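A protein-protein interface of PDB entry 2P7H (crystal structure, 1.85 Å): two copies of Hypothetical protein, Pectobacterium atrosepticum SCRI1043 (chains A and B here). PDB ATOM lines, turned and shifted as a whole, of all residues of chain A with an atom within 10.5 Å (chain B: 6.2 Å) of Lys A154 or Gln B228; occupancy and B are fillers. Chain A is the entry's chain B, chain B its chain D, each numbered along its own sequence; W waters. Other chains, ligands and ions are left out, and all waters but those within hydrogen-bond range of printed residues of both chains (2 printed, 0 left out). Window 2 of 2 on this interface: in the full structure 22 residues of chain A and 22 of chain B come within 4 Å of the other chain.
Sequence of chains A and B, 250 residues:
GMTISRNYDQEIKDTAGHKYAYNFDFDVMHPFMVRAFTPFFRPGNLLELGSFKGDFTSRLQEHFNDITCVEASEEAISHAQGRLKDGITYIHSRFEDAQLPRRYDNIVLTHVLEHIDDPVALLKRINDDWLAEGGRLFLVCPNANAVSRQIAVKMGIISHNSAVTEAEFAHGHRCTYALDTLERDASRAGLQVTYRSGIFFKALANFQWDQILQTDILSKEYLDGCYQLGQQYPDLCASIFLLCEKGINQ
The side-chain amide oxygen (OE1) of Gln B228 lies close to the backbone carbonyl oxygen (O) of Lys A154 (3.3 Å).
The side-chain amide oxygen (OE1) of Gln B232 sits at hydrogen-bond distance from the side-chain amino group (NZ) of Lys A154.
Of chain B, only Gln B228 (3.3 Å) and Gln B232 (2.8 Å) come within 4 Å of Lys A154.
Gln B228 touches one residue of chain A.
Asp B224 touches none of the printed residues of chain A.
Leu B229 touches just these residues of chain A: Val A147 (3.8 Å), Gln A150 (3.6 Å) and Ile A151 (3.8 Å).
No residue of chain A comes within 4 Å of Gln B231.
Printed residues of chain A within 4 Å of Gln B232: Lys A154 (2.8 Å).
Printed residues of chain A within 4 Å of Glu B221: Met A155 (3.4 Å).
Printed residues of chain B within 4 Å of Val A147: Leu B229 (3.8 Å).
Printed residues of chain B within 4 Å of Ile A151: Cys B226 and Leu B229.
The nearest residue of chain B that does not touch Lys A154 is Gly B225 (4.2 Å).
The nearest residue of chain A that does not touch Gln B228 is Met A155 (4.7 Å).
The nearest printed residue of chain A that does not touch Glu B221 is Ile A151 (5.5 Å).
No position is printed for both chains.
Of the 7 pairs that touch across the chains among the printed residues, none has its exchanged pair printed and touching as well.
The backbone carbonyl oxygen (O) of Asn A145 lies within hydrogen-bond range of the side-chain amide nitrogen (NE2) of Gln A150 (2.8 Å).
The backbone carbonyl oxygen (O) of Asp B224 lies close to the side-chain amide nitrogen (NE2) of Gln B228, 3.4 Å away.
Water W1 lies within hydrogen-bond range of the side-chain amide oxygen (OE1) of Gln A150 and the side-chain amide nitrogen (NE2) of Gln B232.
Water W2 lies within hydrogen-bond range of the side-chain amide nitrogen of Gln B232 and the side-chain amino group of Lys A154.
CG1 of Val A147 touches CD2 of Leu B229, 3.8 Å away.
OE1 of Gln A150 touches CD1 of Leu B229, at 3.6 Å.
CD1 of Ile A151 touches SG of Cys B226, at 3.8 Å.
CD2 of Leu B229 touches CG1 of Ile A151, 3.8 Å away.
Met A155 touches Glu B221 (CG to O, 3.4 Å).
Printed residues of chain B that touch a printed residue of chain A: Glu B221, Cys B226, Gln B228, Leu B229 and Gln B232.
Hydrophobic or aromatic side chains of chain B within 4 Å of the printed part of chain A: Leu B229.
Along chain B the printed residues that touch a printed residue of chain A span positions 221 to 232.
Of the 18 printed residues of chain A, 5 touch a printed residue of chain B.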
ATOM      1  N   ALA A 144       5.108  24.302   5.517  1.00  0.00           N
ATOM      2  CA  ALA A 144       5.652  22.943   5.243  1.00  0.00           C
ATOM      3  C   ALA A 144       6.614  22.472   6.333  1.00  0.00           C
ATOM      4  O   ALA A 144       6.673  21.303   6.674  1.00  0.00           O
ATOM      5  CB  ALA A 144       6.384  22.967   3.878  1.00  0.00           C
ATOM      6  N   ASN A 145       7.407  23.396   6.879  1.00  0.00           N
ATOM      7  CA  ASN A 145       8.488  23.036   7.782  1.00  0.00           C
ATOM      8  C   ASN A 145       8.173  23.162   9.290  1.00  0.00           C
ATOM      9  O   ASN A 145       9.092  23.069  10.127  1.00  0.00           O
ATOM     10  CB  ASN A 145       9.743  23.810   7.387  1.00  0.00           C
ATOM     11  CG  ASN A 145      10.226  23.495   5.967  1.00  0.00           C
ATOM     12  OD1 ASN A 145       9.941  22.420   5.410  1.00  0.00           O
ATOM     13  ND2 ASN A 145      10.956  24.429   5.375  1.00  0.00           N
ATOM     14  N   ALA A 146       6.899  23.312   9.621  1.00  0.00           N
ATOM     15  CA  ALA A 146       6.432  23.370  11.010  1.00  0.00           C
ATOM     16  C   ALA A 146       6.985  22.131  11.673  1.00  0.00           C
ATOM     17  O   ALA A 146       6.895  21.033  11.107  1.00  0.00           O
ATOM     18  CB  ALA A 146       4.899  23.324  11.057  1.00  0.00           C
ATOM     19  N   VAL A 147       7.483  22.257  12.888  1.00  0.00           N
ATOM     20  CA  VAL A 147       8.014  21.092  13.616  1.00  0.00           C
ATOM     21  C   VAL A 147       7.008  19.926  13.635  1.00  0.00           C
ATOM     22  O   VAL A 147       7.387  18.805  13.306  1.00  0.00           O
ATOM     23  CB  VAL A 147       8.450  21.437  15.024  1.00  0.00           C
ATOM     24  CG1 VAL A 147       8.744  20.144  15.824  1.00  0.00           C
ATOM     25  CG2 VAL A 147       9.685  22.339  14.936  1.00  0.00           C
ATOM     26  N   SER A 148       5.750  20.212  13.925  1.00  0.00           N
ATOM     27  CA  SER A 148       4.713  19.166  13.975  1.00  0.00           C
ATOM     28  C   SER A 148       4.612  18.386  12.636  1.00  0.00           C
ATOM     29  O   SER A 148       4.472  17.113  12.596  1.00  0.00           O
ATOM     30  CB  SER A 148       3.385  19.801  14.350  1.00  0.00           C
ATOM     31  OG  SER A 148       3.023  20.776  13.402  1.00  0.00           O
ATOM     32  N   ARG A 149       4.695  19.133  11.540  1.00  0.00           N
ATOM     33  CA  ARG A 149       4.615  18.533  10.222  1.00  0.00           C
ATOM     34  C   ARG A 149       5.879  17.708   9.963  1.00  0.00           C
ATOM     35  O   ARG A 149       5.829  16.584   9.442  1.00  0.00           O
ATOM     36  CB  ARG A 149       4.439  19.574   9.133  1.00  0.00           C
ATOM     37  CG  ARG A 149       4.085  18.955   7.803  1.00  0.00           C
ATOM     38  CD  ARG A 149       3.657  19.994   6.785  1.00  0.00           C
ATOM     39  NE  ARG A 149       3.221  19.394   5.508  1.00  0.00           N
ATOM     40  CZ  ARG A 149       1.965  19.069   5.239  1.00  0.00           C
ATOM     41  NH1 ARG A 149       1.042  19.182   6.183  1.00  0.00           N
ATOM     42  NH2 ARG A 149       1.638  18.585   4.054  1.00  0.00           N
ATOM     43  N   GLN A 150       7.028  18.277  10.296  1.00  0.00           N
ATOM     44  CA  GLN A 150       8.258  17.526  10.136  1.00  0.00           C
ATOM     45  C   GLN A 150       8.254  16.198  10.909  1.00  0.00           C
ATOM     46  O   GLN A 150       8.725  15.160  10.437  1.00  0.00           O
ATOM     47  CB  GLN A 150       9.454  18.416  10.503  1.00  0.00           C
ATOM     48  CG  GLN A 150       9.613  19.639   9.664  1.00  0.00           C
ATOM     49  CD  GLN A 150      11.041  20.117   9.620  1.00  0.00           C
ATOM     50  OE1 GLN A 150      11.941  19.356   9.279  1.00  0.00           O
ATOM     51  NE2 GLN A 150      11.262  21.379   9.944  1.00  0.00           N
ATOM     52  N   ILE A 151       7.673  16.205  12.108  1.00  0.00           N
ATOM     53  CA  ILE A 151       7.603  14.992  12.897  1.00  0.00           C
ATOM     54  C   ILE A 151       6.689  13.973  12.171  1.00  0.00           C
ATOM     55  O   ILE A 151       7.027  12.764  12.056  1.00  0.00           O
ATOM     56  CB  ILE A 151       7.152  15.307  14.369  1.00  0.00           C
ATOM     57  CG1 ILE A 151       8.251  16.090  15.093  1.00  0.00           C
ATOM     58  CG2 ILE A 151       6.820  13.986  15.133  1.00  0.00           C
ATOM     59  CD1 ILE A 151       7.757  16.672  16.458  1.00  0.00           C
ATOM     60  N   ALA A 152       5.568  14.459  11.650  1.00  0.00           N
ATOM     61  CA  ALA A 152       4.638  13.619  10.895  1.00  0.00           C
ATOM     62  C   ALA A 152       5.327  12.985   9.670  1.00  0.00           C
ATOM     63  O   ALA A 152       5.088  11.825   9.348  1.00  0.00           O
ATOM     64  CB  ALA A 152       3.441  14.403  10.445  1.00  0.00           C
ATOM     65  N   VAL A 153       6.198  13.754   9.023  1.00  0.00           N
ATOM     66  CA  VAL A 153       6.985  13.276   7.910  1.00  0.00           C
ATOM     67  C   VAL A 153       7.962  12.186   8.389  1.00  0.00           C
ATOM     68  O   VAL A 153       8.049  11.141   7.737  1.00  0.00           O
ATOM     69  CB  VAL A 153       7.727  14.444   7.187  1.00  0.00           C
ATOM     70  CG1 VAL A 153       8.876  13.884   6.288  1.00  0.00           C
ATOM     71  CG2 VAL A 153       6.718  15.342   6.449  1.00  0.00           C
ATOM     72  N   LYS A 154       8.641  12.379   9.535  1.00  0.00           N
ATOM     73  CA  LYS A 154       9.541  11.362  10.092  1.00  0.00           C
ATOM     74  C   LYS A 154       8.795  10.096  10.478  1.00  0.00           C
ATOM     75  O   LYS A 154       9.349   9.006  10.347  1.00  0.00           O
ATOM     76  CB  LYS A 154      10.401  11.886  11.273  1.00  0.00           C
ATOM     77  CG  LYS A 154      11.356  13.025  10.876  1.00  0.00           C
ATOM     78  CD  LYS A 154      12.223  12.646   9.720  1.00  0.00           C
ATOM     79  CE  LYS A 154      13.294  13.672   9.458  1.00  0.00           C
ATOM     80  NZ  LYS A 154      13.919  13.367   8.153  1.00  0.00           N
ATOM     81  N   MET A 155       7.560  10.238  10.931  1.00  0.00           N
ATOM     82  CA  MET A 155       6.694   9.077  11.221  1.00  0.00           C
ATOM     83  C   MET A 155       6.197   8.312   9.980  1.00  0.00           C
ATOM     84  O   MET A 155       5.650   7.212  10.104  1.00  0.00           O
ATOM     85  CB  MET A 155       5.482   9.519  12.059  1.00  0.00           C
ATOM     86  CG  MET A 155       5.817  10.077  13.428  1.00  0.00           C
ATOM     87  SD  MET A 155       4.229  11.012  14.139  1.00  0.00           S
ATOM     88  CE  MET A 155       3.142   9.408  14.533  1.00  0.00           C
ATOM     89  N   GLY A 156       6.365   8.869   8.794  1.00  0.00           N
ATOM     90  CA  GLY A 156       5.912   8.233   7.569  1.00  0.00           C
ATOM     91  C   GLY A 156       4.475   8.513   7.245  1.00  0.00           C
ATOM     92  O   GLY A 156       3.958   7.970   6.275  1.00  0.00           O
ATOM     93  N   ILE A 157       3.841   9.409   8.013  1.00  0.00           N
ATOM     94  CA  ILE A 157       2.442   9.760   7.772  1.00  0.00           C
ATOM     95  C   ILE A 157       2.300  10.635   6.529  1.00  0.00           C
ATOM     96  O   ILE A 157       1.312  10.513   5.787  1.00  0.00           O
ATOM     97  CB  ILE A 157       1.836  10.483   8.994  1.00  0.00           C
ATOM     98  CG1 ILE A 157       1.812   9.529  10.181  1.00  0.00           C
ATOM     99  CG2 ILE A 157       0.434  10.989   8.650  1.00  0.00           C
ATOM    100  CD1 ILE A 157       1.444  10.198  11.420  1.00  0.00           C
ATOM    101  N   ILE A 158       3.275  11.529   6.337  1.00  0.00           N
ATOM    102  CA  ILE A 158       3.320  12.489   5.190  1.00  0.00           C
ATOM    103  C   ILE A 158       4.616  12.238   4.436  1.00  0.00           C
ATOM    104  O   ILE A 158       5.641  12.077   5.060  1.00  0.00           O
ATOM    105  CB  ILE A 158       3.249  13.980   5.643  1.00  0.00           C
ATOM    106  CG1 ILE A 158       1.983  14.210   6.497  1.00  0.00           C
ATOM    107  CG2 ILE A 158       3.312  14.953   4.443  1.00  0.00           C
ATOM    108  CD1 ILE A 158       1.844  15.621   7.128  1.00  0.00           C
ATOM    109  N   SER A 159       4.590  12.188   3.117  1.00  0.00           N
ATOM    110  CA  SER A 159       5.793  11.755   2.370  1.00  0.00           C
ATOM    111  C   SER A 159       7.007  12.680   2.567  1.00  0.00           C
ATOM    112  O   SER A 159       8.133  12.218   2.725  1.00  0.00           O
ATOM    113  CB  SER A 159       5.502  11.636   0.884  1.00  0.00           C
ATOM    114  OG  SER A 159       5.112  12.849   0.283  1.00  0.00           O
ATOM    115  N   HIS A 160       6.763  13.982   2.466  1.00  0.00           N
ATOM    116  CA  HIS A 160       7.763  14.989   2.665  1.00  0.00           C
ATOM    117  C   HIS A 160       7.121  16.320   3.036  1.00  0.00           C
ATOM    118  O   HIS A 160       5.901  16.493   2.945  1.00  0.00           O
ATOM    119  CB  HIS A 160       8.645  15.153   1.428  1.00  0.00           C
ATOM    120  CG  HIS A 160       7.922  15.568   0.198  1.00  0.00           C
ATOM    121  ND1 HIS A 160       7.148  14.693  -0.543  1.00  0.00           N
ATOM    122  CD2 HIS A 160       7.928  16.747  -0.480  1.00  0.00           C
ATOM    123  CE1 HIS A 160       6.659  15.344  -1.594  1.00  0.00           C
ATOM    124  NE2 HIS A 160       7.123  16.592  -1.579  1.00  0.00           N
ATOM    125  N   ASN A 161       7.949  17.263   3.473  1.00  0.00           N
ATOM    126  CA  ASN A 161       7.404  18.467   4.138  1.00  0.00           C
ATOM    127  C   ASN A 161       6.437  19.239   3.231  1.00  0.00           C
ATOM    128  O   ASN A 161       5.378  19.638   3.662  1.00  0.00           O
ATOM    129  CB  ASN A 161       8.541  19.407   4.580  1.00  0.00           C
ATOM    130  CG  ASN A 161       9.435  18.826   5.675  1.00  0.00           C
ATOM    131  OD1 ASN A 161       9.317  17.669   6.072  1.00  0.00           O
ATOM    132  ND2 ASN A 161      10.385  19.655   6.140  1.00  0.00           N
ATOM    133  N   ARG B  35      19.657   4.257  21.854  1.00  0.00           N
ATOM    134  CA  ARG B  35      19.555   4.315  20.389  1.00  0.00           C
ATOM    135  C   ARG B  35      20.600   5.264  19.779  1.00  0.00           C
ATOM    136  O   ARG B  35      21.250   4.909  18.813  1.00  0.00           O
ATOM    137  CB  ARG B  35      18.119   4.680  19.910  1.00  0.00           C
ATOM    138  CG  ARG B  35      17.307   3.499  19.340  1.00  0.00           C
ATOM    139  CD  ARG B  35      15.924   3.907  18.764  1.00  0.00           C
ATOM    140  NE  ARG B  35      15.950   4.488  17.409  1.00  0.00           N
ATOM    141  CZ  ARG B  35      14.899   5.050  16.797  1.00  0.00           C
ATOM    142  NH1 ARG B  35      13.718   5.128  17.402  1.00  0.00           N
ATOM    143  NH2 ARG B  35      15.019   5.548  15.568  1.00  0.00           N
ATOM    144  N   GLU B 221       5.112   6.322  18.274  1.00  0.00           N
ATOM    145  CA  GLU B 221       5.658   6.737  16.971  1.00  0.00           C
ATOM    146  C   GLU B 221       5.927   8.225  16.966  1.00  0.00           C
ATOM    147  O   GLU B 221       6.902   8.666  16.333  1.00  0.00           O
ATOM    148  CB  GLU B 221       4.740   6.378  15.834  1.00  0.00           C
ATOM    149  CG  GLU B 221       4.639   4.885  15.584  1.00  0.00           C
ATOM    150  CD  GLU B 221       3.683   4.168  16.545  1.00  0.00           C
ATOM    151  OE1 GLU B 221       2.920   4.845  17.310  1.00  0.00           O
ATOM    152  OE2 GLU B 221       3.712   2.913  16.528  1.00  0.00           O
ATOM    153  N   LEU B 223       6.928   9.914  19.564  1.00  0.00           N
ATOM    154  CA  LEU B 223       8.197  10.045  20.288  1.00  0.00           C
ATOM    155  C   LEU B 223       9.373   9.617  19.410  1.00  0.00           C
ATOM    156  O   LEU B 223      10.410  10.251  19.426  1.00  0.00           O
ATOM    157  CB  LEU B 223       8.144   9.224  21.573  1.00  0.00           C
ATOM    158  CG  LEU B 223       7.093   9.643  22.625  1.00  0.00           C
ATOM    159  CD1 LEU B 223       7.120   8.638  23.774  1.00  0.00           C
ATOM    160  CD2 LEU B 223       7.318  11.076  23.139  1.00  0.00           C
ATOM    161  N   ASP B 224       9.226   8.562  18.631  1.00  0.00           N
ATOM    162  CA  ASP B 224      10.288   8.166  17.661  1.00  0.00           C
ATOM    163  C   ASP B 224      10.540   9.287  16.663  1.00  0.00           C
ATOM    164  O   ASP B 224      11.675   9.597  16.365  1.00  0.00           O
ATOM    165  CB  ASP B 224       9.910   6.895  16.883  1.00  0.00           C
ATOM    166  CG  ASP B 224      10.023   5.625  17.727  1.00  0.00           C
ATOM    167  OD1 ASP B 224      10.652   5.661  18.808  1.00  0.00           O
ATOM    168  OD2 ASP B 224       9.475   4.588  17.285  1.00  0.00           O
ATOM    169  N   GLY B 225       9.470   9.911  16.167  1.00  0.00           N
ATOM    170  CA  GLY B 225       9.587  11.092  15.317  1.00  0.00           C
ATOM    171  C   GLY B 225      10.354  12.241  15.931  1.00  0.00           C
ATOM    172  O   GLY B 225      11.144  12.910  15.239  1.00  0.00           O
ATOM    173  N   CYS B 226      10.152  12.487  17.220  1.00  0.00           N
ATOM    174  CA  CYS B 226      10.887  13.544  17.910  1.00  0.00           C
ATOM    175  C   CYS B 226      12.382  13.224  17.964  1.00  0.00           C
ATOM    176  O   CYS B 226      13.227  14.127  17.956  1.00  0.00           O
ATOM    177  CB  CYS B 226      10.350  13.742  19.341  1.00  0.00           C
ATOM    178  SG  CYS B 226       8.677  14.446  19.399  1.00  0.00           S
ATOM    179  N   TYR B 227      12.699  11.941  18.129  1.00  0.00           N
ATOM    180  CA  TYR B 227      14.072  11.477  18.154  1.00  0.00           C
ATOM    181  C   TYR B 227      14.739  11.690  16.790  1.00  0.00           C
ATOM    182  O   TYR B 227      15.870  12.213  16.692  1.00  0.00           O
ATOM    183  CB  TYR B 227      14.177  10.022  18.632  1.00  0.00           C
ATOM    184  CG  TYR B 227      15.538   9.396  18.406  1.00  0.00           C
ATOM    185  CD1 TYR B 227      16.619   9.718  19.220  1.00  0.00           C
ATOM    186  CD2 TYR B 227      15.761   8.521  17.355  1.00  0.00           C
ATOM    187  CE1 TYR B 227      17.876   9.166  18.995  1.00  0.00           C
ATOM    188  CE2 TYR B 227      17.024   8.003  17.110  1.00  0.00           C
ATOM    189  CZ  TYR B 227      18.062   8.296  17.943  1.00  0.00           C
ATOM    190  OH  TYR B 227      19.309   7.715  17.688  1.00  0.00           O
ATOM    191  N   GLN B 228      14.039  11.286  15.750  1.00  0.00           N
ATOM    192  CA  GLN B 228      14.580  11.368  14.400  1.00  0.00           C
ATOM    193  C   GLN B 228      14.772  12.823  14.002  1.00  0.00           C
ATOM    194  O   GLN B 228      15.814  13.193  13.481  1.00  0.00           O
ATOM    195  CB  GLN B 228      13.632  10.717  13.436  1.00  0.00           C
ATOM    196  CG  GLN B 228      13.455   9.234  13.572  1.00  0.00           C
ATOM    197  CD  GLN B 228      12.334   8.786  12.652  1.00  0.00           C
ATOM    198  OE1 GLN B 228      12.440   8.856  11.418  1.00  0.00           O
ATOM    199  NE2 GLN B 228      11.228   8.446  13.239  1.00  0.00           N
ATOM    200  N   LEU B 229      13.780  13.660  14.298  1.00  0.00           N
ATOM    201  CA  LEU B 229      13.891  15.088  13.996  1.00  0.00           C
ATOM    202  C   LEU B 229      14.977  15.780  14.832  1.00  0.00           C
ATOM    203  O   LEU B 229      15.663  16.659  14.332  1.00  0.00           O
ATOM    204  CB  LEU B 229      12.562  15.842  14.163  1.00  0.00           C
ATOM    205  CG  LEU B 229      12.557  17.290  13.629  1.00  0.00           C
ATOM    206  CD1 LEU B 229      12.733  17.266  12.121  1.00  0.00           C
ATOM    207  CD2 LEU B 229      11.297  18.008  14.040  1.00  0.00           C
ATOM    208  N   GLY B 230      15.157  15.379  16.078  1.00  0.00           N
ATOM    209  CA  GLY B 230      16.145  15.999  16.960  1.00  0.00           C
ATOM    210  C   GLY B 230      17.574  15.908  16.413  1.00  0.00           C
ATOM    211  O   GLY B 230      18.413  16.802  16.636  1.00  0.00           O
ATOM    212  N   GLN B 231      17.864  14.825  15.691  1.00  0.00           N
ATOM    213  CA  GLN B 231      19.171  14.679  15.035  1.00  0.00           C
ATOM    214  C   GLN B 231      19.439  15.764  14.017  1.00  0.00           C
ATOM    215  O   GLN B 231      20.592  16.110  13.803  1.00  0.00           O
ATOM    216  CB  GLN B 231      19.275  13.336  14.323  1.00  0.00           C
ATOM    217  CG  GLN B 231      19.260  12.143  15.296  1.00  0.00           C
ATOM    218  CD  GLN B 231      19.649  10.845  14.655  1.00  0.00           C
ATOM    219  OE1 GLN B 231      19.540  10.660  13.441  1.00  0.00           O
ATOM    220  NE2 GLN B 231      20.134   9.921  15.480  1.00  0.00           N
ATOM    221  N   GLN B 232      18.380  16.295  13.404  1.00  0.00           N
ATOM    222  CA  GLN B 232      18.502  17.388  12.449  1.00  0.00           C
ATOM    223  C   GLN B 232      18.593  18.756  13.068  1.00  0.00           C
ATOM    224  O   GLN B 232      18.948  19.691  12.383  1.00  0.00           O
ATOM    225  CB  GLN B 232      17.343  17.344  11.499  1.00  0.00           C
ATOM    226  CG  GLN B 232      17.384  16.015  10.756  1.00  0.00           C
ATOM    227  CD  GLN B 232      16.297  15.837   9.760  1.00  0.00           C
ATOM    228  OE1 GLN B 232      16.174  14.738   9.227  1.00  0.00           O
ATOM    229  NE2 GLN B 232      15.518  16.902   9.459  1.00  0.00           N
HETATM  230  O   HOH W   1      14.701  19.893   8.867  1.00  0.00           O
HETATM  231  O   HOH W   2      13.495  16.537   7.494  1.00  0.00           O
